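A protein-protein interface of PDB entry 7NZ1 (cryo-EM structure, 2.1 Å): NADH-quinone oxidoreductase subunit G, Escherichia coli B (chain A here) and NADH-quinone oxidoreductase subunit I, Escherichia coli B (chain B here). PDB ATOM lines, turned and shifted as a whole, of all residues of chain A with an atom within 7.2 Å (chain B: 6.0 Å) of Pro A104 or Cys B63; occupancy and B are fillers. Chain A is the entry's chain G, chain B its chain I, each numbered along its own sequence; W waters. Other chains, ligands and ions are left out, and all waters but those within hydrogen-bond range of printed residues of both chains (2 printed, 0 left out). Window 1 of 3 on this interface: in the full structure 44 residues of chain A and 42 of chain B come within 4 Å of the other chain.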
ATOM      1  N   HIS A 101     -29.915   4.061 -38.030  1.00  0.00           N
ATOM      2  CA  HIS A 101     -29.419   4.869 -36.915  1.00  0.00           C
ATOM      3  C   HIS A 101     -29.839   4.214 -35.592  1.00  0.00           C
ATOM      4  O   HIS A 101     -30.641   4.742 -34.821  1.00  0.00           O
ATOM      5  CB  HIS A 101     -29.979   6.279 -37.067  1.00  0.00           C
ATOM      6  CG  HIS A 101     -29.284   7.328 -36.258  1.00  0.00           C
ATOM      7  ND1 HIS A 101     -28.239   8.075 -36.756  1.00  0.00           N
ATOM      8  CD2 HIS A 101     -29.524   7.801 -35.014  1.00  0.00           C
ATOM      9  CE1 HIS A 101     -27.841   8.938 -35.840  1.00  0.00           C
ATOM     10  NE2 HIS A 101     -28.605   8.792 -34.773  1.00  0.00           N
ATOM     11  N   ASP A 102     -29.266   3.039 -35.324  1.00  0.00           N
ATOM     12  CA  ASP A 102     -29.802   2.159 -34.293  1.00  0.00           C
ATOM     13  C   ASP A 102     -28.881   1.816 -33.131  1.00  0.00           C
ATOM     14  O   ASP A 102     -29.342   1.106 -32.233  1.00  0.00           O
ATOM     15  CB  ASP A 102     -30.266   0.833 -34.910  1.00  0.00           C
ATOM     16  CG  ASP A 102     -31.611   0.929 -35.583  1.00  0.00           C
ATOM     17  OD1 ASP A 102     -32.216   2.019 -35.588  1.00  0.00           O
ATOM     18  OD2 ASP A 102     -32.068  -0.107 -36.100  1.00  0.00           O
ATOM     19  N   CYS A 103     -27.632   2.294 -33.115  1.00  0.00           N
ATOM     20  CA  CYS A 103     -26.657   1.917 -32.081  1.00  0.00           C
ATOM     21  C   CYS A 103     -27.074   2.109 -30.615  1.00  0.00           C
ATOM     22  O   CYS A 103     -26.726   1.229 -29.811  1.00  0.00           O
ATOM     23  CB  CYS A 103     -25.319   2.640 -32.309  1.00  0.00           C
ATOM     24  SG  CYS A 103     -24.502   2.343 -33.856  1.00  0.00           S
ATOM     25  N   PRO A 104     -27.770   3.189 -30.190  1.00  0.00           N
ATOM     26  CA  PRO A 104     -28.282   3.214 -28.806  1.00  0.00           C
ATOM     27  C   PRO A 104     -29.262   2.104 -28.457  1.00  0.00           C
ATOM     28  O   PRO A 104     -29.274   1.652 -27.310  1.00  0.00           O
ATOM     29  CB  PRO A 104     -28.958   4.586 -28.724  1.00  0.00           C
ATOM     30  CG  PRO A 104     -28.198   5.382 -29.636  1.00  0.00           C
ATOM     31  CD  PRO A 104     -27.998   4.517 -30.801  1.00  0.00           C
ATOM     32  N   VAL A 105     -30.081   1.653 -29.400  1.00  0.00           N
ATOM     33  CA  VAL A 105     -31.066   0.614 -29.133  1.00  0.00           C
ATOM     34  C   VAL A 105     -30.712  -0.690 -29.848  1.00  0.00           C
ATOM     35  O   VAL A 105     -31.581  -1.514 -30.095  1.00  0.00           O
ATOM     36  CB  VAL A 105     -32.488   1.079 -29.483  1.00  0.00           C
ATOM     37  CG1 VAL A 105     -32.920   2.178 -28.552  1.00  0.00           C
ATOM     38  CG2 VAL A 105     -32.560   1.548 -30.929  1.00  0.00           C
ATOM     39  N   CYS A 106     -29.443  -0.887 -30.177  1.00  0.00           N
ATOM     40  CA  CYS A 106     -28.968  -2.137 -30.753  1.00  0.00           C
ATOM     41  C   CYS A 106     -28.244  -2.930 -29.678  1.00  0.00           C
ATOM     42  O   CYS A 106     -27.366  -2.395 -28.994  1.00  0.00           O
ATOM     43  CB  CYS A 106     -28.039  -1.882 -31.943  1.00  0.00           C
ATOM     44  SG  CYS A 106     -27.570  -3.344 -32.888  1.00  0.00           S
ATOM     45  N   GLU A 107     -28.595  -4.209 -29.544  1.00  0.00           N
ATOM     46  CA  GLU A 107     -27.953  -5.048 -28.536  1.00  0.00           C
ATOM     47  C   GLU A 107     -26.517  -5.411 -28.894  1.00  0.00           C
ATOM     48  O   GLU A 107     -25.781  -5.881 -28.025  1.00  0.00           O
ATOM     49  CB  GLU A 107     -28.767  -6.320 -28.304  1.00  0.00           C
ATOM     50  CG  GLU A 107     -30.178  -6.069 -27.822  1.00  0.00           C
ATOM     51  CD  GLU A 107     -31.207  -6.207 -28.922  1.00  0.00           C
ATOM     52  OE1 GLU A 107     -31.006  -5.631 -30.015  1.00  0.00           O
ATOM     53  OE2 GLU A 107     -32.223  -6.895 -28.694  1.00  0.00           O
ATOM     54  N   GLY A 109     -24.333  -3.148 -29.751  1.00  0.00           N
ATOM     55  CA  GLY A 109     -23.551  -1.963 -29.424  1.00  0.00           C
ATOM     56  C   GLY A 109     -22.525  -2.096 -28.313  1.00  0.00           C
ATOM     57  O   GLY A 109     -22.851  -2.497 -27.195  1.00  0.00           O
ATOM     58  N   GLN A 115     -18.981  -1.724 -35.915  1.00  0.00           N
ATOM     59  CA  GLN A 115     -18.562  -0.510 -35.216  1.00  0.00           C
ATOM     60  C   GLN A 115     -17.045  -0.407 -35.140  1.00  0.00           C
ATOM     61  O   GLN A 115     -16.482   0.679 -35.308  1.00  0.00           O
ATOM     62  CB  GLN A 115     -19.140  -0.480 -33.801  1.00  0.00           C
ATOM     63  CG  GLN A 115     -20.588  -0.066 -33.673  1.00  0.00           C
ATOM     64  CD  GLN A 115     -20.980   0.163 -32.225  1.00  0.00           C
ATOM     65  OE1 GLN A 115     -20.439  -0.471 -31.322  1.00  0.00           O
ATOM     66  NE2 GLN A 115     -21.919   1.067 -31.999  1.00  0.00           N
ATOM     67  N   TYR A 215     -30.930  -6.721 -20.505  1.00  0.00           N
ATOM     68  CA  TYR A 215     -29.793  -6.325 -21.322  1.00  0.00           C
ATOM     69  C   TYR A 215     -28.830  -5.465 -20.517  1.00  0.00           C
ATOM     70  O   TYR A 215     -29.245  -4.652 -19.688  1.00  0.00           O
ATOM     71  CB  TYR A 215     -30.235  -5.566 -22.580  1.00  0.00           C
ATOM     72  CG  TYR A 215     -29.065  -5.216 -23.473  1.00  0.00           C
ATOM     73  CD1 TYR A 215     -28.414  -6.201 -24.209  1.00  0.00           C
ATOM     74  CD2 TYR A 215     -28.560  -3.917 -23.521  1.00  0.00           C
ATOM     75  CE1 TYR A 215     -27.318  -5.896 -24.993  1.00  0.00           C
ATOM     76  CE2 TYR A 215     -27.467  -3.606 -24.297  1.00  0.00           C
ATOM     77  CZ  TYR A 215     -26.851  -4.598 -25.035  1.00  0.00           C
ATOM     78  OH  TYR A 215     -25.765  -4.285 -25.809  1.00  0.00           O
ATOM     79  N   ARG A 217     -24.651  -3.669 -21.458  1.00  0.00           N
ATOM     80  CA  ARG A 217     -23.538  -3.591 -22.385  1.00  0.00           C
ATOM     81  C   ARG A 217     -22.364  -4.428 -21.886  1.00  0.00           C
ATOM     82  O   ARG A 217     -22.302  -4.828 -20.722  1.00  0.00           O
ATOM     83  CB  ARG A 217     -23.120  -2.139 -22.573  1.00  0.00           C
ATOM     84  CG  ARG A 217     -24.254  -1.247 -22.997  1.00  0.00           C
ATOM     85  CD  ARG A 217     -24.377  -1.260 -24.490  1.00  0.00           C
ATOM     86  NE  ARG A 217     -25.438  -0.381 -24.954  1.00  0.00           N
ATOM     87  CZ  ARG A 217     -26.075  -0.525 -26.104  1.00  0.00           C
ATOM     88  NH1 ARG A 217     -25.783  -1.510 -26.933  1.00  0.00           N
ATOM     89  NH2 ARG A 217     -27.029   0.337 -26.429  1.00  0.00           N
ATOM     90  N   TRP A 219     -19.164  -3.712 -21.459  1.00  0.00           N
ATOM     91  CA  TRP A 219     -18.252  -3.103 -20.498  1.00  0.00           C
ATOM     92  C   TRP A 219     -18.757  -3.180 -19.058  1.00  0.00           C
ATOM     93  O   TRP A 219     -17.947  -3.097 -18.135  1.00  0.00           O
ATOM     94  CB  TRP A 219     -17.979  -1.649 -20.873  1.00  0.00           C
ATOM     95  CG  TRP A 219     -19.183  -0.776 -21.116  1.00  0.00           C
ATOM     96  CD1 TRP A 219     -19.989  -0.224 -20.172  1.00  0.00           C
ATOM     97  CD2 TRP A 219     -19.691  -0.330 -22.381  1.00  0.00           C
ATOM     98  NE1 TRP A 219     -20.975   0.522 -20.758  1.00  0.00           N
ATOM     99  CE2 TRP A 219     -20.814   0.479 -22.115  1.00  0.00           C
ATOM    100  CE3 TRP A 219     -19.313  -0.543 -23.709  1.00  0.00           C
ATOM    101  CZ2 TRP A 219     -21.557   1.077 -23.126  1.00  0.00           C
ATOM    102  CZ3 TRP A 219     -20.058   0.043 -24.709  1.00  0.00           C
ATOM    103  CH2 TRP A 219     -21.171   0.841 -24.414  1.00  0.00           C
ATOM    104  N   CYS B  60     -35.103   8.908 -22.716  1.00  0.00           N
ATOM    105  CA  CYS B  60     -33.998   8.002 -22.450  1.00  0.00           C
ATOM    106  C   CYS B  60     -34.319   6.621 -23.003  1.00  0.00           C
ATOM    107  O   CYS B  60     -35.402   6.083 -22.768  1.00  0.00           O
ATOM    108  CB  CYS B  60     -33.727   7.943 -20.946  1.00  0.00           C
ATOM    109  SG  CYS B  60     -32.438   6.806 -20.415  1.00  0.00           S
ATOM    110  N   VAL B  61     -33.379   6.054 -23.749  1.00  0.00           N
ATOM    111  CA  VAL B  61     -33.554   4.739 -24.344  1.00  0.00           C
ATOM    112  C   VAL B  61     -32.700   3.697 -23.646  1.00  0.00           C
ATOM    113  O   VAL B  61     -32.565   2.579 -24.149  1.00  0.00           O
ATOM    114  CB  VAL B  61     -33.281   4.763 -25.857  1.00  0.00           C
ATOM    115  CG1 VAL B  61     -34.191   5.755 -26.529  1.00  0.00           C
ATOM    116  CG2 VAL B  61     -31.826   5.105 -26.150  1.00  0.00           C
ATOM    117  N   ALA B  62     -32.121   4.057 -22.492  1.00  0.00           N
ATOM    118  CA  ALA B  62     -31.348   3.173 -21.613  1.00  0.00           C
ATOM    119  C   ALA B  62     -30.154   2.533 -22.326  1.00  0.00           C
ATOM    120  O   ALA B  62     -29.841   1.359 -22.132  1.00  0.00           O
ATOM    121  CB  ALA B  62     -32.242   2.120 -20.961  1.00  0.00           C
ATOM    122  N   CYS B  63     -29.492   3.326 -23.163  1.00  0.00           N
ATOM    123  CA  CYS B  63     -28.338   2.908 -23.944  1.00  0.00           C
ATOM    124  C   CYS B  63     -27.051   2.792 -23.135  1.00  0.00           C
ATOM    125  O   CYS B  63     -26.073   2.257 -23.668  1.00  0.00           O
ATOM    126  CB  CYS B  63     -28.133   3.891 -25.099  1.00  0.00           C
ATOM    127  SG  CYS B  63     -27.255   5.401 -24.650  1.00  0.00           S
ATOM    128  N   ASN B  64     -27.029   3.307 -21.898  1.00  0.00           N
ATOM    129  CA  ASN B  64     -25.924   3.212 -20.935  1.00  0.00           C
ATOM    130  C   ASN B  64     -24.651   3.927 -21.396  1.00  0.00           C
ATOM    131  O   ASN B  64     -23.562   3.607 -20.921  1.00  0.00           O
ATOM    132  CB  ASN B  64     -25.593   1.756 -20.563  1.00  0.00           C
ATOM    133  CG  ASN B  64     -26.197   1.337 -19.247  1.00  0.00           C
ATOM    134  OD1 ASN B  64     -27.227   0.671 -19.210  1.00  0.00           O
ATOM    135  ND2 ASN B  64     -25.557   1.721 -18.157  1.00  0.00           N
ATOM    136  N   LEU B  65     -24.744   4.910 -22.294  1.00  0.00           N
ATOM    137  CA  LEU B  65     -23.546   5.658 -22.669  1.00  0.00           C
ATOM    138  C   LEU B  65     -23.203   6.731 -21.646  1.00  0.00           C
ATOM    139  O   LEU B  65     -22.025   7.034 -21.446  1.00  0.00           O
ATOM    140  CB  LEU B  65     -23.706   6.312 -24.040  1.00  0.00           C
ATOM    141  CG  LEU B  65     -23.561   5.466 -25.301  1.00  0.00           C
ATOM    142  CD1 LEU B  65     -23.717   6.357 -26.506  1.00  0.00           C
ATOM    143  CD2 LEU B  65     -22.219   4.762 -25.327  1.00  0.00           C
ATOM    144  N   CYS B  66     -24.218   7.321 -21.015  1.00  0.00           N
ATOM    145  CA  CYS B  66     -23.994   8.310 -19.969  1.00  0.00           C
ATOM    146  C   CYS B  66     -23.323   7.695 -18.745  1.00  0.00           C
ATOM    147  O   CYS B  66     -22.478   8.338 -18.115  1.00  0.00           O
ATOM    148  CB  CYS B  66     -25.323   8.960 -19.593  1.00  0.00           C
ATOM    149  SG  CYS B  66     -26.496   7.821 -18.827  1.00  0.00           S
ATOM    150  N   LEU B  77     -28.183   2.283 -14.253  1.00  0.00           N
ATOM    151  CA  LEU B  77     -29.483   2.121 -14.893  1.00  0.00           C
ATOM    152  C   LEU B  77     -29.602   0.732 -15.507  1.00  0.00           C
ATOM    153  O   LEU B  77     -28.606   0.041 -15.725  1.00  0.00           O
ATOM    154  CB  LEU B  77     -29.717   3.213 -15.946  1.00  0.00           C
ATOM    155  CG  LEU B  77     -28.793   3.234 -17.155  1.00  0.00           C
ATOM    156  CD1 LEU B  77     -29.573   2.896 -18.386  1.00  0.00           C
ATOM    157  CD2 LEU B  77     -28.103   4.571 -17.304  1.00  0.00           C
ATOM    158  N   TRP B  87     -37.301   0.761 -26.056  1.00  0.00           N
ATOM    159  CA  TRP B  87     -36.369   0.730 -24.934  1.00  0.00           C
ATOM    160  C   TRP B  87     -36.594   1.932 -24.016  1.00  0.00           C
ATOM    161  O   TRP B  87     -36.751   3.063 -24.481  1.00  0.00           O
ATOM    162  CB  TRP B  87     -34.922   0.741 -25.428  1.00  0.00           C
ATOM    163  CG  TRP B  87     -34.409  -0.481 -26.142  1.00  0.00           C
ATOM    164  CD1 TRP B  87     -35.123  -1.395 -26.862  1.00  0.00           C
ATOM    165  CD2 TRP B  87     -33.047  -0.915 -26.187  1.00  0.00           C
ATOM    166  NE1 TRP B  87     -34.289  -2.360 -27.358  1.00  0.00           N
ATOM    167  CE2 TRP B  87     -33.006  -2.084 -26.969  1.00  0.00           C
ATOM    168  CE3 TRP B  87     -31.855  -0.422 -25.648  1.00  0.00           C
ATOM    169  CZ2 TRP B  87     -31.826  -2.787 -27.194  1.00  0.00           C
ATOM    170  CZ3 TRP B  87     -30.682  -1.109 -25.894  1.00  0.00           C
ATOM    171  CH2 TRP B  87     -30.676  -2.276 -26.662  1.00  0.00           C
ATOM    172  N   CYS B 109     -24.798  11.750 -24.354  1.00  0.00           N
ATOM    173  CA  CYS B 109     -26.144  11.244 -24.633  1.00  0.00           C
ATOM    174  C   CYS B 109     -26.537  11.404 -26.095  1.00  0.00           C
ATOM    175  O   CYS B 109     -26.533  12.525 -26.608  1.00  0.00           O
ATOM    176  CB  CYS B 109     -27.167  11.950 -23.763  1.00  0.00           C
ATOM    177  SG  CYS B 109     -28.848  11.281 -23.874  1.00  0.00           S
ATOM    178  N   PRO B 110     -26.899  10.336 -26.783  1.00  0.00           N
ATOM    179  CA  PRO B 110     -27.295  10.454 -28.189  1.00  0.00           C
ATOM    180  C   PRO B 110     -28.787  10.669 -28.391  1.00  0.00           C
ATOM    181  O   PRO B 110     -29.292  10.494 -29.500  1.00  0.00           O
ATOM    182  CB  PRO B 110     -26.840   9.115 -28.768  1.00  0.00           C
ATOM    183  CG  PRO B 110     -27.011   8.167 -27.620  1.00  0.00           C
ATOM    184  CD  PRO B 110     -26.889   8.932 -26.336  1.00  0.00           C
ATOM    185  N   THR B 111     -29.513  11.031 -27.332  1.00  0.00           N
ATOM    186  CA  THR B 111     -30.938  11.324 -27.437  1.00  0.00           C
ATOM    187  C   THR B 111     -31.317  12.672 -26.843  1.00  0.00           C
ATOM    188  O   THR B 111     -32.499  13.025 -26.891  1.00  0.00           O
ATOM    189  CB  THR B 111     -31.800  10.243 -26.749  1.00  0.00           C
ATOM    190  OG1 THR B 111     -31.577  10.276 -25.338  1.00  0.00           O
ATOM    191  CG2 THR B 111     -31.531   8.842 -27.286  1.00  0.00           C
ATOM    192  N   PHE B 150     -35.368  10.980 -31.062  1.00  0.00           N
ATOM    193  CA  PHE B 150     -34.389  10.010 -31.541  1.00  0.00           C
ATOM    194  C   PHE B 150     -35.044   8.897 -32.352  1.00  0.00           C
ATOM    195  O   PHE B 150     -34.455   8.415 -33.327  1.00  0.00           O
ATOM    196  CB  PHE B 150     -33.616   9.423 -30.349  1.00  0.00           C
ATOM    197  CG  PHE B 150     -32.924   8.110 -30.640  1.00  0.00           C
ATOM    198  CD1 PHE B 150     -31.710   8.098 -31.310  1.00  0.00           C
ATOM    199  CD2 PHE B 150     -33.462   6.895 -30.216  1.00  0.00           C
ATOM    200  CE1 PHE B 150     -31.063   6.907 -31.584  1.00  0.00           C
ATOM    201  CE2 PHE B 150     -32.823   5.705 -30.493  1.00  0.00           C
ATOM    202  CZ  PHE B 150     -31.620   5.713 -31.174  1.00  0.00           C
HETATM  203  O   HOH W   1     -25.139  -1.770 -19.321  1.00  0.00           O
HETATM  204  O   HOH W   2     -29.038  10.023 -32.192  1.00  0.00           O
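The backbone carbonyl oxygen (O) of Cys B63 sits at hydrogen-bond distance from the guanidinium group (NE) of Arg A217.
The backbone carbonyl oxygen (O) of Pro A104 lies within hydrogen-bond range of the guanidinium group (NH2) of Arg A217 (2.7 Å).
The backbone carbonyl oxygen of Cys A106 is in hydrogen-bond range of the guanidinium group of Arg A217.
OH of Tyr A215 is in hydrogen-bond range of O of Glu A107 (2.7 Å).
The backbone carbonyl oxygen of Gly A109 is in hydrogen-bond range of the guanidinium group of Arg A217 (3.1 Å).
OH of Tyr A215 sits at hydrogen-bond distance from NH1 of Arg A217 (3.0 Å).
The side-chain sulfur (SG) of Cys B63 lies close to the backbone NH (N) of Leu B65 (3.5 Å).
Among the printed residues, merely in contact across the chains: His A101 with Phe B150, Pro A104 with Val B61, Pro A104 with Cys B63, Pro A104 with Trp B87, Pro A104 with Pro B110, Pro A104 with Phe B150, Val A105 with Val B61, Val A105 with Trp B87, Cys A106 with Trp B87, Glu A107 with Trp B87, Arg A217 with Trp B87 and Trp A219 with Asn B64.
Of chain B, only Val B61, Cys B63, Trp B87, Pro B110 and Phe B150 come within 4 Å of Pro A104.
Cys B63 touches two residues of chain A.
Of the printed residues of chain B, Arg A217 touches Cys B63 (3.0 Å) and Trp B87 (3.97 Å).
Of the printed residues of chain B, Trp A219 touches Asn B64.
Printed residues of chain B within 4 Å of Glu A107: Trp B87 (3.7 Å).
Printed residues of chain B within 4 Å of His A101: Phe B150.
Cys B60 touches none of the printed residues of chain A.
The nearest residue of chain B that does not touch Pro A104 is Ala B62 (5.1 Å).
The nearest printed residue of chain B that does not touch Val A105 is Phe B150 (4.03 Å).
Of the 13 printed residues of chain B, 6 touch a printed residue of chain A.
Hydrophobic or aromatic side chains of chain B that line the printed part of chain A: Val B61, Trp B87, Pro B110 and Phe B150.
Of the 12 printed residues of chain A, 7 touch a printed residue of chain B.
Hydrophobic or aromatic side chains of chain A that line the printed part of chain B: His A101, Pro A104, Val A105 and Trp A219.
Among the printed residues, 13 pairs touch across the chains.
Among the printed residues, no Asp or Glu carboxylate lies within 4 Å of a Lys or Arg side-chain nitrogen of the other chain.
Water W2 lies within hydrogen-bond range of O of Pro B110 and NE2 of His A101.
Water W1 bridges N of Arg A217 (2.9 Å) and OD1 of Asn B64 (3.2 Å).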
